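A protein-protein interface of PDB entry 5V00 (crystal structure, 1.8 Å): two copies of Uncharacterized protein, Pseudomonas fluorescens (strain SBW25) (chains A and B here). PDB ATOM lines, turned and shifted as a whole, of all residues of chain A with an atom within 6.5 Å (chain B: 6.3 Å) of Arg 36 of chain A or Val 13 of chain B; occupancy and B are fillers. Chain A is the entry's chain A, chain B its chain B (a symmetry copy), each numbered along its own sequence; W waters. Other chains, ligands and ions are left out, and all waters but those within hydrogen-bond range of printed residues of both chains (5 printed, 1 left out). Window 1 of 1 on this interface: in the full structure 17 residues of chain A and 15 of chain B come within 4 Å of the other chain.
Water W2 lies within hydrogen-bond range of OD2 of Asp 18 of chain B (2.7 Å), N of Arg 15 of chain B (2.9 Å) and NH1 of Arg 36 of chain A (2.9 Å). Water W4 bridges OD1 of Asp 18 of chain B and O of Phe 45 of chain A. Water W1 lies within hydrogen-bond range of the backbone carbonyl oxygen of Asp 37 of chain A (2.8 Å), the backbone NH of Val 13 of chain B (2.9 Å) and the backbone carbonyl oxygen of Arg 36 of chain A (3.1 Å). Water W5 lies within hydrogen-bond range of the side-chain hydroxyl of Ser 12 of chain B and the backbone carbonyl oxygen of Arg 36 of chain A. Water W3 bridges the guanidinium group (NH1) of Arg 36 of chain A (3.1 Å) and the backbone carbonyl oxygen (O) of Arg 15 of chain B (3.1 Å).
Trp 14 of chain B touches Glu 33 of chain A (CZ3 to OE2, 3.8 Å). Val 13 of chain B touches Arg 36 of chain A (O to CD, 3.9 Å). Trp 14 of chain B touches Arg 36 of chain A (CZ3 to NE, 3.6 Å). O of Ala 38 of chain A touches CB of Val 13 of chain B, 3.5 Å away. OE1 of Glu 159 of chain B touches CB of Ala 38 of chain A, 3.5 Å away.
Arg 36 of chain A touches just these residues of chain B: Val 13 (3.9 Å) and Trp 14 (3.6 Å). Of the printed residues of chain A, Val 13 of chain B touches Arg 36 (3.9 Å) and Ala 38 (3.5 Å). Of the printed residues of chain B, Gly 39 of chain A touches Arg 15. Of the printed residues of chain B, Phe 45 of chain A touches Asp 18. Of the printed residues of chain B, Ala 38 of chain A touches Val 13 (3.5 Å), Arg 15 (2.9 Å) and Glu 159 (3.5 Å). Leu 167 of chain B touches none of the printed residues of chain A. Ile 11 of chain B touches none of the printed residues of chain A. The nearest residue of chain B that does not touch Arg 36 of chain A is Asp 18 of chain B (4.1 Å). The nearest residue of chain A that does not touch Val 13 of chain B is Asp 37 of chain A (4.1 Å). The nearest printed residue of chain B that does not touch Glu 33 of chain A is Ser 12 of chain B (6.3 Å).
Printed residues of chain A that touch a printed residue of chain B: Glu 33, Arg 36, Ala 38, Gly 39 and Phe 45. Hydrophobic or aromatic side chains of chain A within 4 Å of the printed part of chain B: Ala 38 and Phe 45. Of the 13 printed residues of chain B, 5 touch a printed residue of chain A. Printed residues of chain B that touch a printed residue of chain A: Val 13, Trp 14, Arg 15, Asp 18 and Glu 159. Along chain B the printed residues that touch a printed residue of chain A span positions 13 to 159. Among the printed residues, no Asp or Glu carboxylate lies within 4 Å of a Lys or Arg side-chain nitrogen of the other chain.
The backbone NH of Phe 45 of chain A lies within hydrogen-bond range of the side-chain carboxylate of Asp 18 of chain B (2.8 Å). NE of Arg 15 of chain B lies within hydrogen-bond range of O of Ala 38 of chain A, 2.9 Å away. NH2 of Arg 15 of chain B lies within hydrogen-bond range of O of Gly 39 of chain A, 3.2 Å away.
Position printed for both chains: 168. Of the 8 pairs that touch across the chains among the printed residues, none has its exchanged pair printed and touching as well.
The side-chain carboxylate (OD1) of Asp 37 of chain A sits close to the backbone NH (N) of Gly 39 of chain A (3.3 Å). The guanidinium group (NH1) of Arg 15 of chain B lies within salt-bridge range of the side-chain carboxylate (OD2) of Asp 165 of chain B. OE1 of Glu 33 of chain A is in salt-bridge range of NH2 of Arg 36 of chain A (2.9 Å). NE1 of Trp 14 of chain B is in hydrogen-bond range of OE1 of Gln 168 of chain B, 2.8 Å away. The guanidinium group (NH1) of Arg 15 of chain B lies within hydrogen-bond range of the backbone carbonyl oxygen (O) of Lys 160 of chain B, 2.8 Å away. N of Trp 14 of chain B lies within hydrogen-bond range of O of Cys 166 of chain B (2.8 Å).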
ATOM      1  N   GLU A  33     -21.454  -5.507 -13.054  1.00  0.00           N
ATOM      2  CA  GLU A  33     -20.352  -6.147 -12.353  1.00  0.00           C
ATOM      3  C   GLU A  33     -20.690  -7.599 -12.036  1.00  0.00           C
ATOM      4  O   GLU A  33     -21.720  -7.928 -11.382  1.00  0.00           O
ATOM      5  CB  GLU A  33     -20.109  -5.418 -10.998  1.00  0.00           C
ATOM      6  CG  GLU A  33     -19.059  -6.068 -10.122  1.00  0.00           C
ATOM      7  CD  GLU A  33     -17.651  -5.791 -10.584  1.00  0.00           C
ATOM      8  OE1 GLU A  33     -17.407  -5.061 -11.615  1.00  0.00           O
ATOM      9  OE2 GLU A  33     -16.757  -6.347  -9.910  1.00  0.00           O
ATOM     10  N   ILE A  34     -19.793  -8.512 -12.393  1.00  0.00           N
ATOM     11  CA  ILE A  34     -19.882  -9.867 -11.943  1.00  0.00           C
ATOM     12  C   ILE A  34     -18.976 -10.110 -10.726  1.00  0.00           C
ATOM     13  O   ILE A  34     -19.481 -10.379  -9.571  1.00  0.00           O
ATOM     14  CB  ILE A  34     -19.548 -10.931 -13.044  1.00  0.00           C
ATOM     15  CG1 ILE A  34     -20.474 -10.688 -14.228  1.00  0.00           C
ATOM     16  CG2 ILE A  34     -19.698 -12.320 -12.461  1.00  0.00           C
ATOM     17  CD1 ILE A  34     -20.163 -11.603 -15.397  1.00  0.00           C
ATOM     18  N   THR A  35     -17.658  -9.963 -10.885  1.00  0.00           N
ATOM     19  CA  THR A  35     -16.704 -10.215  -9.814  1.00  0.00           C
ATOM     20  C   THR A  35     -15.347  -9.670 -10.229  1.00  0.00           C
ATOM     21  O   THR A  35     -15.145  -9.458 -11.433  1.00  0.00           O
ATOM     22  CB  THR A  35     -16.617 -11.732  -9.467  1.00  0.00           C
ATOM     23  OG1 THR A  35     -15.758 -11.919  -8.348  1.00  0.00           O
ATOM     24  CG2 THR A  35     -16.115 -12.539 -10.618  1.00  0.00           C
ATOM     25  N   ARG A  36     -14.486  -9.347  -9.263  1.00  0.00           N
ATOM     26  CA  ARG A  36     -13.177  -8.828  -9.523  1.00  0.00           C
ATOM     27  C   ARG A  36     -12.273  -9.257  -8.383  1.00  0.00           C
ATOM     28  O   ARG A  36     -12.765  -9.743  -7.347  1.00  0.00           O
ATOM     29  CB  ARG A  36     -13.161  -7.362  -9.737  1.00  0.00           C
ATOM     30  CG  ARG A  36     -13.548  -6.544  -8.443  1.00  0.00           C
ATOM     31  CD  ARG A  36     -13.438  -5.056  -8.684  1.00  0.00           C
ATOM     32  NE  ARG A  36     -14.472  -4.560  -9.576  1.00  0.00           N
ATOM     33  CZ  ARG A  36     -14.695  -3.285  -9.854  1.00  0.00           C
ATOM     34  NH1 ARG A  36     -13.886  -2.317  -9.389  1.00  0.00           N
ATOM     35  NH2 ARG A  36     -15.725  -2.981 -10.603  1.00  0.00           N
ATOM     36  N   ASP A  37     -10.971  -9.188  -8.598  1.00  0.00           N
ATOM     37  CA  ASP A  37     -10.030  -9.524  -7.519  1.00  0.00           C
ATOM     38  C   ASP A  37     -10.013  -8.428  -6.440  1.00  0.00           C
ATOM     39  O   ASP A  37     -10.740  -7.436  -6.543  1.00  0.00           O
ATOM     40  CB  ASP A  37      -8.626  -9.870  -7.992  1.00  0.00           C
ATOM     41  CG  ASP A  37      -7.801  -8.659  -8.352  1.00  0.00           C
ATOM     42  OD1 ASP A  37      -8.410  -7.655  -8.762  1.00  0.00           O
ATOM     43  OD2 ASP A  37      -6.561  -8.759  -8.130  1.00  0.00           O
ATOM     44  N   ALA A  38      -9.199  -8.654  -5.439  1.00  0.00           N
ATOM     45  CA  ALA A  38      -9.135  -7.624  -4.396  1.00  0.00           C
ATOM     46  C   ALA A  38      -8.350  -6.431  -4.788  1.00  0.00           C
ATOM     47  O   ALA A  38      -8.457  -5.355  -4.191  1.00  0.00           O
ATOM     48  CB  ALA A  38      -8.526  -8.197  -3.123  1.00  0.00           C
ATOM     49  N   GLY A  39      -7.531  -6.540  -5.820  1.00  0.00           N
ATOM     50  CA  GLY A  39      -6.806  -5.350  -6.318  1.00  0.00           C
ATOM     51  C   GLY A  39      -5.683  -4.867  -5.399  1.00  0.00           C
ATOM     52  O   GLY A  39      -5.366  -5.506  -4.379  1.00  0.00           O
ATOM     53  N   PHE A  45      -8.030  -3.014  -9.523  1.00  0.00           N
ATOM     54  CA  PHE A  45      -8.215  -4.429  -9.762  1.00  0.00           C
ATOM     55  C   PHE A  45      -7.097  -4.952 -10.645  1.00  0.00           C
ATOM     56  O   PHE A  45      -6.580  -4.184 -11.472  1.00  0.00           O
ATOM     57  CB  PHE A  45      -9.595  -4.768 -10.318  1.00  0.00           C
ATOM     58  CG  PHE A  45      -9.909  -4.191 -11.678  1.00  0.00           C
ATOM     59  CD1 PHE A  45      -9.325  -4.726 -12.823  1.00  0.00           C
ATOM     60  CD2 PHE A  45     -10.806  -3.170 -11.822  1.00  0.00           C
ATOM     61  CE1 PHE A  45      -9.573  -4.088 -14.092  1.00  0.00           C
ATOM     62  CE2 PHE A  45     -11.158  -2.648 -13.082  1.00  0.00           C
ATOM     63  CZ  PHE A  45     -10.487  -3.080 -14.206  1.00  0.00           C
ATOM     64  N   TRP A  47      -7.853  -8.176 -11.980  1.00  0.00           N
ATOM     65  CA  TRP A  47      -8.744  -8.822 -12.967  1.00  0.00           C
ATOM     66  C   TRP A  47     -10.154  -8.463 -12.654  1.00  0.00           C
ATOM     67  O   TRP A  47     -10.543  -8.186 -11.477  1.00  0.00           O
ATOM     68  CB  TRP A  47      -8.564 -10.362 -13.061  1.00  0.00           C
ATOM     69  CG  TRP A  47      -8.771 -11.190 -11.831  1.00  0.00           C
ATOM     70  CD1 TRP A  47      -7.798 -11.767 -11.093  1.00  0.00           C
ATOM     71  CD2 TRP A  47     -10.010 -11.621 -11.291  1.00  0.00           C
ATOM     72  NE1 TRP A  47      -8.360 -12.547 -10.100  1.00  0.00           N
ATOM     73  CE2 TRP A  47      -9.727 -12.438 -10.188  1.00  0.00           C
ATOM     74  CE3 TRP A  47     -11.338 -11.389 -11.642  1.00  0.00           C
ATOM     75  CZ2 TRP A  47     -10.764 -13.015  -9.381  1.00  0.00           C
ATOM     76  CZ3 TRP A  47     -12.329 -11.975 -10.864  1.00  0.00           C
ATOM     77  CH2 TRP A  47     -12.016 -12.769  -9.772  1.00  0.00           C
ATOM     78  N   ARG A  48     -10.988  -8.494 -13.689  1.00  0.00           N
ATOM     79  CA  ARG A  48     -12.422  -8.193 -13.555  1.00  0.00           C
ATOM     80  C   ARG A  48     -13.240  -8.977 -14.565  1.00  0.00           C
ATOM     81  O   ARG A  48     -12.785  -9.084 -15.726  1.00  0.00           O
ATOM     82  CB  ARG A  48     -12.662  -6.683 -13.671  1.00  0.00           C
ATOM     83  CG  ARG A  48     -14.129  -6.269 -13.614  1.00  0.00           C
ATOM     84  CD  ARG A  48     -14.355  -4.829 -14.032  1.00  0.00           C
ATOM     85  NE  ARG A  48     -15.749  -4.473 -13.705  1.00  0.00           N
ATOM     86  CZ  ARG A  48     -16.405  -3.394 -14.103  1.00  0.00           C
ATOM     87  NH1 ARG A  48     -15.822  -2.558 -14.938  1.00  0.00           N
ATOM     88  NH2 ARG A  48     -17.615  -3.158 -13.675  1.00  0.00           N
ATOM     89  N   LEU A  49     -14.365  -9.534 -14.155  1.00  0.00           N
ATOM     90  CA  LEU A  49     -15.405 -10.047 -15.063  1.00  0.00           C
ATOM     91  C   LEU A  49     -16.615  -9.173 -15.001  1.00  0.00           C
ATOM     92  O   LEU A  49     -17.121  -8.801 -13.879  1.00  0.00           O
ATOM     93  CB  LEU A  49     -15.786 -11.465 -14.685  1.00  0.00           C
ATOM     94  CG  LEU A  49     -14.958 -12.627 -15.053  1.00  0.00           C
ATOM     95  CD1 LEU A  49     -13.563 -12.614 -14.549  1.00  0.00           C
ATOM     96  CD2 LEU A  49     -15.691 -13.930 -14.639  1.00  0.00           C
ATOM     97  N   GLN A 168     -17.546 -19.219  -8.731  1.00  0.00           N
ATOM     98  CA  GLN A 168     -16.165 -18.860  -8.441  1.00  0.00           C
ATOM     99  C   GLN A 168     -15.577 -19.770  -7.386  1.00  0.00           C
ATOM    100  O   GLN A 168     -16.153 -19.861  -6.267  1.00  0.00           O
ATOM    101  CB  GLN A 168     -16.104 -17.409  -8.001  1.00  0.00           C
ATOM    102  CG  GLN A 168     -14.748 -16.880  -7.660  1.00  0.00           C
ATOM    103  CD  GLN A 168     -14.677 -15.367  -7.527  1.00  0.00           C
ATOM    104  OE1 GLN A 168     -15.512 -14.615  -8.043  1.00  0.00           O
ATOM    105  NE2 GLN A 168     -13.609 -14.912  -6.870  1.00  0.00           N
ATOM    106  N   ILE B  11     -16.730 -11.342  -0.177  1.00  0.00           N
ATOM    107  CA  ILE B  11     -16.000 -10.101   0.051  1.00  0.00           C
ATOM    108  C   ILE B  11     -15.623  -9.486  -1.255  1.00  0.00           C
ATOM    109  O   ILE B  11     -15.094 -10.203  -2.148  1.00  0.00           O
ATOM    110  CB  ILE B  11     -14.742 -10.357   0.907  1.00  0.00           C
ATOM    111  CG1 ILE B  11     -15.177 -10.861   2.303  1.00  0.00           C
ATOM    112  CG2 ILE B  11     -13.883  -9.100   1.033  1.00  0.00           C
ATOM    113  CD1 ILE B  11     -14.021 -11.552   3.053  1.00  0.00           C
ATOM    114  N   SER B  12     -15.896  -8.205  -1.427  1.00  0.00           N
ATOM    115  CA  SER B  12     -15.460  -7.433  -2.594  1.00  0.00           C
ATOM    116  C   SER B  12     -14.608  -6.266  -2.136  1.00  0.00           C
ATOM    117  O   SER B  12     -14.847  -5.725  -1.074  1.00  0.00           O
ATOM    118  CB  SER B  12     -16.682  -6.921  -3.306  1.00  0.00           C
ATOM    119  OG  SER B  12     -17.426  -7.944  -3.895  1.00  0.00           O
ATOM    120  N   VAL B  13     -13.586  -5.853  -2.893  1.00  0.00           N
ATOM    121  CA  VAL B  13     -12.803  -4.679  -2.576  1.00  0.00           C
ATOM    122  C   VAL B  13     -12.936  -3.728  -3.789  1.00  0.00           C
ATOM    123  O   VAL B  13     -12.636  -4.116  -4.940  1.00  0.00           O
ATOM    124  CB  VAL B  13     -11.331  -4.947  -2.248  1.00  0.00           C
ATOM    125  CG1 VAL B  13     -10.579  -3.666  -1.940  1.00  0.00           C
ATOM    126  CG2 VAL B  13     -11.214  -5.978  -1.124  1.00  0.00           C
ATOM    127  N   TRP B  14     -13.467  -2.516  -3.557  1.00  0.00           N
ATOM    128  CA  TRP B  14     -13.638  -1.484  -4.584  1.00  0.00           C
ATOM    129  C   TRP B  14     -12.403  -0.593  -4.416  1.00  0.00           C
ATOM    130  O   TRP B  14     -12.196   0.055  -3.320  1.00  0.00           O
ATOM    131  CB  TRP B  14     -14.942  -0.706  -4.362  1.00  0.00           C
ATOM    132  CG  TRP B  14     -16.164  -1.534  -4.174  1.00  0.00           C
ATOM    133  CD1 TRP B  14     -16.925  -1.718  -3.053  1.00  0.00           C
ATOM    134  CD2 TRP B  14     -16.687  -2.420  -5.135  1.00  0.00           C
ATOM    135  NE1 TRP B  14     -17.944  -2.591  -3.287  1.00  0.00           N
ATOM    136  CE2 TRP B  14     -17.795  -3.075  -4.559  1.00  0.00           C
ATOM    137  CE3 TRP B  14     -16.263  -2.798  -6.402  1.00  0.00           C
ATOM    138  CZ2 TRP B  14     -18.517  -4.056  -5.215  1.00  0.00           C
ATOM    139  CZ3 TRP B  14     -16.998  -3.788  -7.072  1.00  0.00           C
ATOM    140  CH2 TRP B  14     -18.124  -4.403  -6.458  1.00  0.00           C
ATOM    141  N   ARG B  15     -11.547  -0.519  -5.429  1.00  0.00           N
ATOM    142  CA  ARG B  15     -10.380   0.316  -5.337  1.00  0.00           C
ATOM    143  C   ARG B  15     -10.668   1.690  -5.942  1.00  0.00           C
ATOM    144  O   ARG B  15     -11.241   1.831  -7.032  1.00  0.00           O
ATOM    145  CB  ARG B  15      -9.135  -0.269  -5.971  1.00  0.00           C
ATOM    146  CG  ARG B  15      -8.694  -1.609  -5.437  1.00  0.00           C
ATOM    147  CD  ARG B  15      -8.133  -1.437  -3.982  1.00  0.00           C
ATOM    148  NE  ARG B  15      -7.680  -2.692  -3.525  1.00  0.00           N
ATOM    149  CZ  ARG B  15      -7.098  -2.892  -2.324  1.00  0.00           C
ATOM    150  NH1 ARG B  15      -6.888  -1.826  -1.551  1.00  0.00           N
ATOM    151  NH2 ARG B  15      -6.811  -4.083  -1.923  1.00  0.00           N
ATOM    152  N   ASP B  18     -10.114   2.726  -9.562  1.00  0.00           N
ATOM    153  CA  ASP B  18     -11.095   2.299 -10.544  1.00  0.00           C
ATOM    154  C   ASP B  18     -12.365   3.076 -10.617  1.00  0.00           C
ATOM    155  O   ASP B  18     -13.233   2.827 -11.480  1.00  0.00           O
ATOM    156  CB  ASP B  18     -11.398   0.809 -10.340  1.00  0.00           C
ATOM    157  CG  ASP B  18     -10.140  -0.041 -10.428  1.00  0.00           C
ATOM    158  OD1 ASP B  18      -9.292   0.139 -11.366  1.00  0.00           O
ATOM    159  OD2 ASP B  18      -9.939  -0.971  -9.582  1.00  0.00           O
ATOM    160  N   GLU B 159      -7.618  -7.842   4.156  1.00  0.00           N
ATOM    161  CA  GLU B 159      -7.361  -6.899   3.084  1.00  0.00           C
ATOM    162  C   GLU B 159      -6.791  -5.633   3.684  1.00  0.00           C
ATOM    163  O   GLU B 159      -6.900  -5.362   4.919  1.00  0.00           O
ATOM    164  CB  GLU B 159      -8.634  -6.636   2.319  1.00  0.00           C
ATOM    165  CG  GLU B 159      -9.296  -7.832   1.717  1.00  0.00           C
ATOM    166  CD  GLU B 159      -8.444  -8.601   0.697  1.00  0.00           C
ATOM    167  OE1 GLU B 159      -7.489  -8.070   0.168  1.00  0.00           O
ATOM    168  OE2 GLU B 159      -8.823  -9.771   0.488  1.00  0.00           O
ATOM    169  N   LYS B 160      -6.129  -4.884   2.832  1.00  0.00           N
ATOM    170  CA  LYS B 160      -5.576  -3.619   3.150  1.00  0.00           C
ATOM    171  C   LYS B 160      -6.144  -2.561   2.213  1.00  0.00           C
ATOM    172  O   LYS B 160      -5.953  -2.585   0.981  1.00  0.00           O
ATOM    173  CB  LYS B 160      -4.049  -3.658   3.020  1.00  0.00           C
ATOM    174  CG  LYS B 160      -3.405  -4.573   4.046  1.00  0.00           C
ATOM    175  CD  LYS B 160      -1.883  -4.483   3.921  1.00  0.00           C
ATOM    176  CE  LYS B 160      -1.249  -5.308   5.041  1.00  0.00           C
ATOM    177  NZ  LYS B 160       0.240  -5.271   4.961  1.00  0.00           N
ATOM    178  N   LEU B 161      -6.830  -1.589   2.791  1.00  0.00           N
ATOM    179  CA  LEU B 161      -7.475  -0.545   2.069  1.00  0.00           C
ATOM    180  C   LEU B 161      -6.707   0.751   2.188  1.00  0.00           C
ATOM    181  O   LEU B 161      -6.422   1.242   3.294  1.00  0.00           O
ATOM    182  CB  LEU B 161      -8.856  -0.317   2.648  1.00  0.00           C
ATOM    183  CG  LEU B 161      -9.759  -1.505   2.855  1.00  0.00           C
ATOM    184  CD1 LEU B 161     -11.079  -1.011   3.413  1.00  0.00           C
ATOM    185  CD2 LEU B 161     -10.003  -2.114   1.481  1.00  0.00           C
ATOM    186  N   ASP B 165     -10.534   3.539  -0.693  1.00  0.00           N
ATOM    187  CA  ASP B 165     -10.873   2.175  -1.071  1.00  0.00           C
ATOM    188  C   ASP B 165     -11.995   1.691  -0.130  1.00  0.00           C
ATOM    189  O   ASP B 165     -12.118   2.216   1.012  1.00  0.00           O
ATOM    190  CB  ASP B 165      -9.655   1.247  -0.935  1.00  0.00           C
ATOM    191  CG  ASP B 165      -8.521   1.524  -1.912  1.00  0.00           C
ATOM    192  OD1 ASP B 165      -8.738   2.192  -2.968  1.00  0.00           O
ATOM    193  OD2 ASP B 165      -7.397   1.046  -1.626  1.00  0.00           O
ATOM    194  N   CYS B 166     -12.822   0.756  -0.583  1.00  0.00           N
ATOM    195  CA  CYS B 166     -13.969   0.277   0.205  1.00  0.00           C
ATOM    196  C   CYS B 166     -14.123  -1.225   0.129  1.00  0.00           C
ATOM    197  O   CYS B 166     -14.160  -1.756  -0.956  1.00  0.00           O
ATOM    198  CB  CYS B 166     -15.234   0.922  -0.382  1.00  0.00           C
ATOM    199  SG  CYS B 166     -16.760   0.650   0.492  1.00  0.00           S
ATOM    200  N   LEU B 167     -14.209  -1.904   1.278  1.00  0.00           N
ATOM    201  CA  LEU B 167     -14.492  -3.305   1.349  1.00  0.00           C
ATOM    202  C   LEU B 167     -15.965  -3.484   1.539  1.00  0.00           C
ATOM    203  O   LEU B 167     -16.635  -2.682   2.236  1.00  0.00           O
ATOM    204  CB  LEU B 167     -13.727  -3.895   2.513  1.00  0.00           C
ATOM    205  CG  LEU B 167     -13.899  -5.389   2.669  1.00  0.00           C
ATOM    206  CD1 LEU B 167     -12.604  -6.081   2.999  1.00  0.00           C
ATOM    207  CD2 LEU B 167     -14.989  -5.727   3.653  1.00  0.00           C
ATOM    208  N   GLN B 168     -16.548  -4.479   0.865  1.00  0.00           N
ATOM    209  CA  GLN B 168     -17.960  -4.811   0.953  1.00  0.00           C
ATOM    210  C   GLN B 168     -18.144  -6.304   1.229  1.00  0.00           C
ATOM    211  O   GLN B 168     -17.567  -7.141   0.522  1.00  0.00           O
ATOM    212  CB  GLN B 168     -18.692  -4.479  -0.311  1.00  0.00           C
ATOM    213  CG  GLN B 168     -20.162  -4.830  -0.339  1.00  0.00           C
ATOM    214  CD  GLN B 168     -20.929  -4.215  -1.530  1.00  0.00           C
ATOM    215  OE1 GLN B 168     -20.448  -3.311  -2.198  1.00  0.00           O
ATOM    216  NE2 GLN B 168     -22.195  -4.598  -1.655  1.00  0.00           N
HETATM  217  O   HOH W   1     -13.044  -7.818  -4.955  1.00  0.00           O
HETATM  218  O   HOH W   2     -11.466  -2.195  -7.777  1.00  0.00           O
HETATM  219  O   HOH W   3     -13.836   0.303  -7.823  1.00  0.00           O
HETATM  220  O   HOH W   4      -7.419  -1.617 -12.421  1.00  0.00           O
HETATM  221  O   HOH W   5     -15.560  -8.769  -6.084  1.00  0.00           O
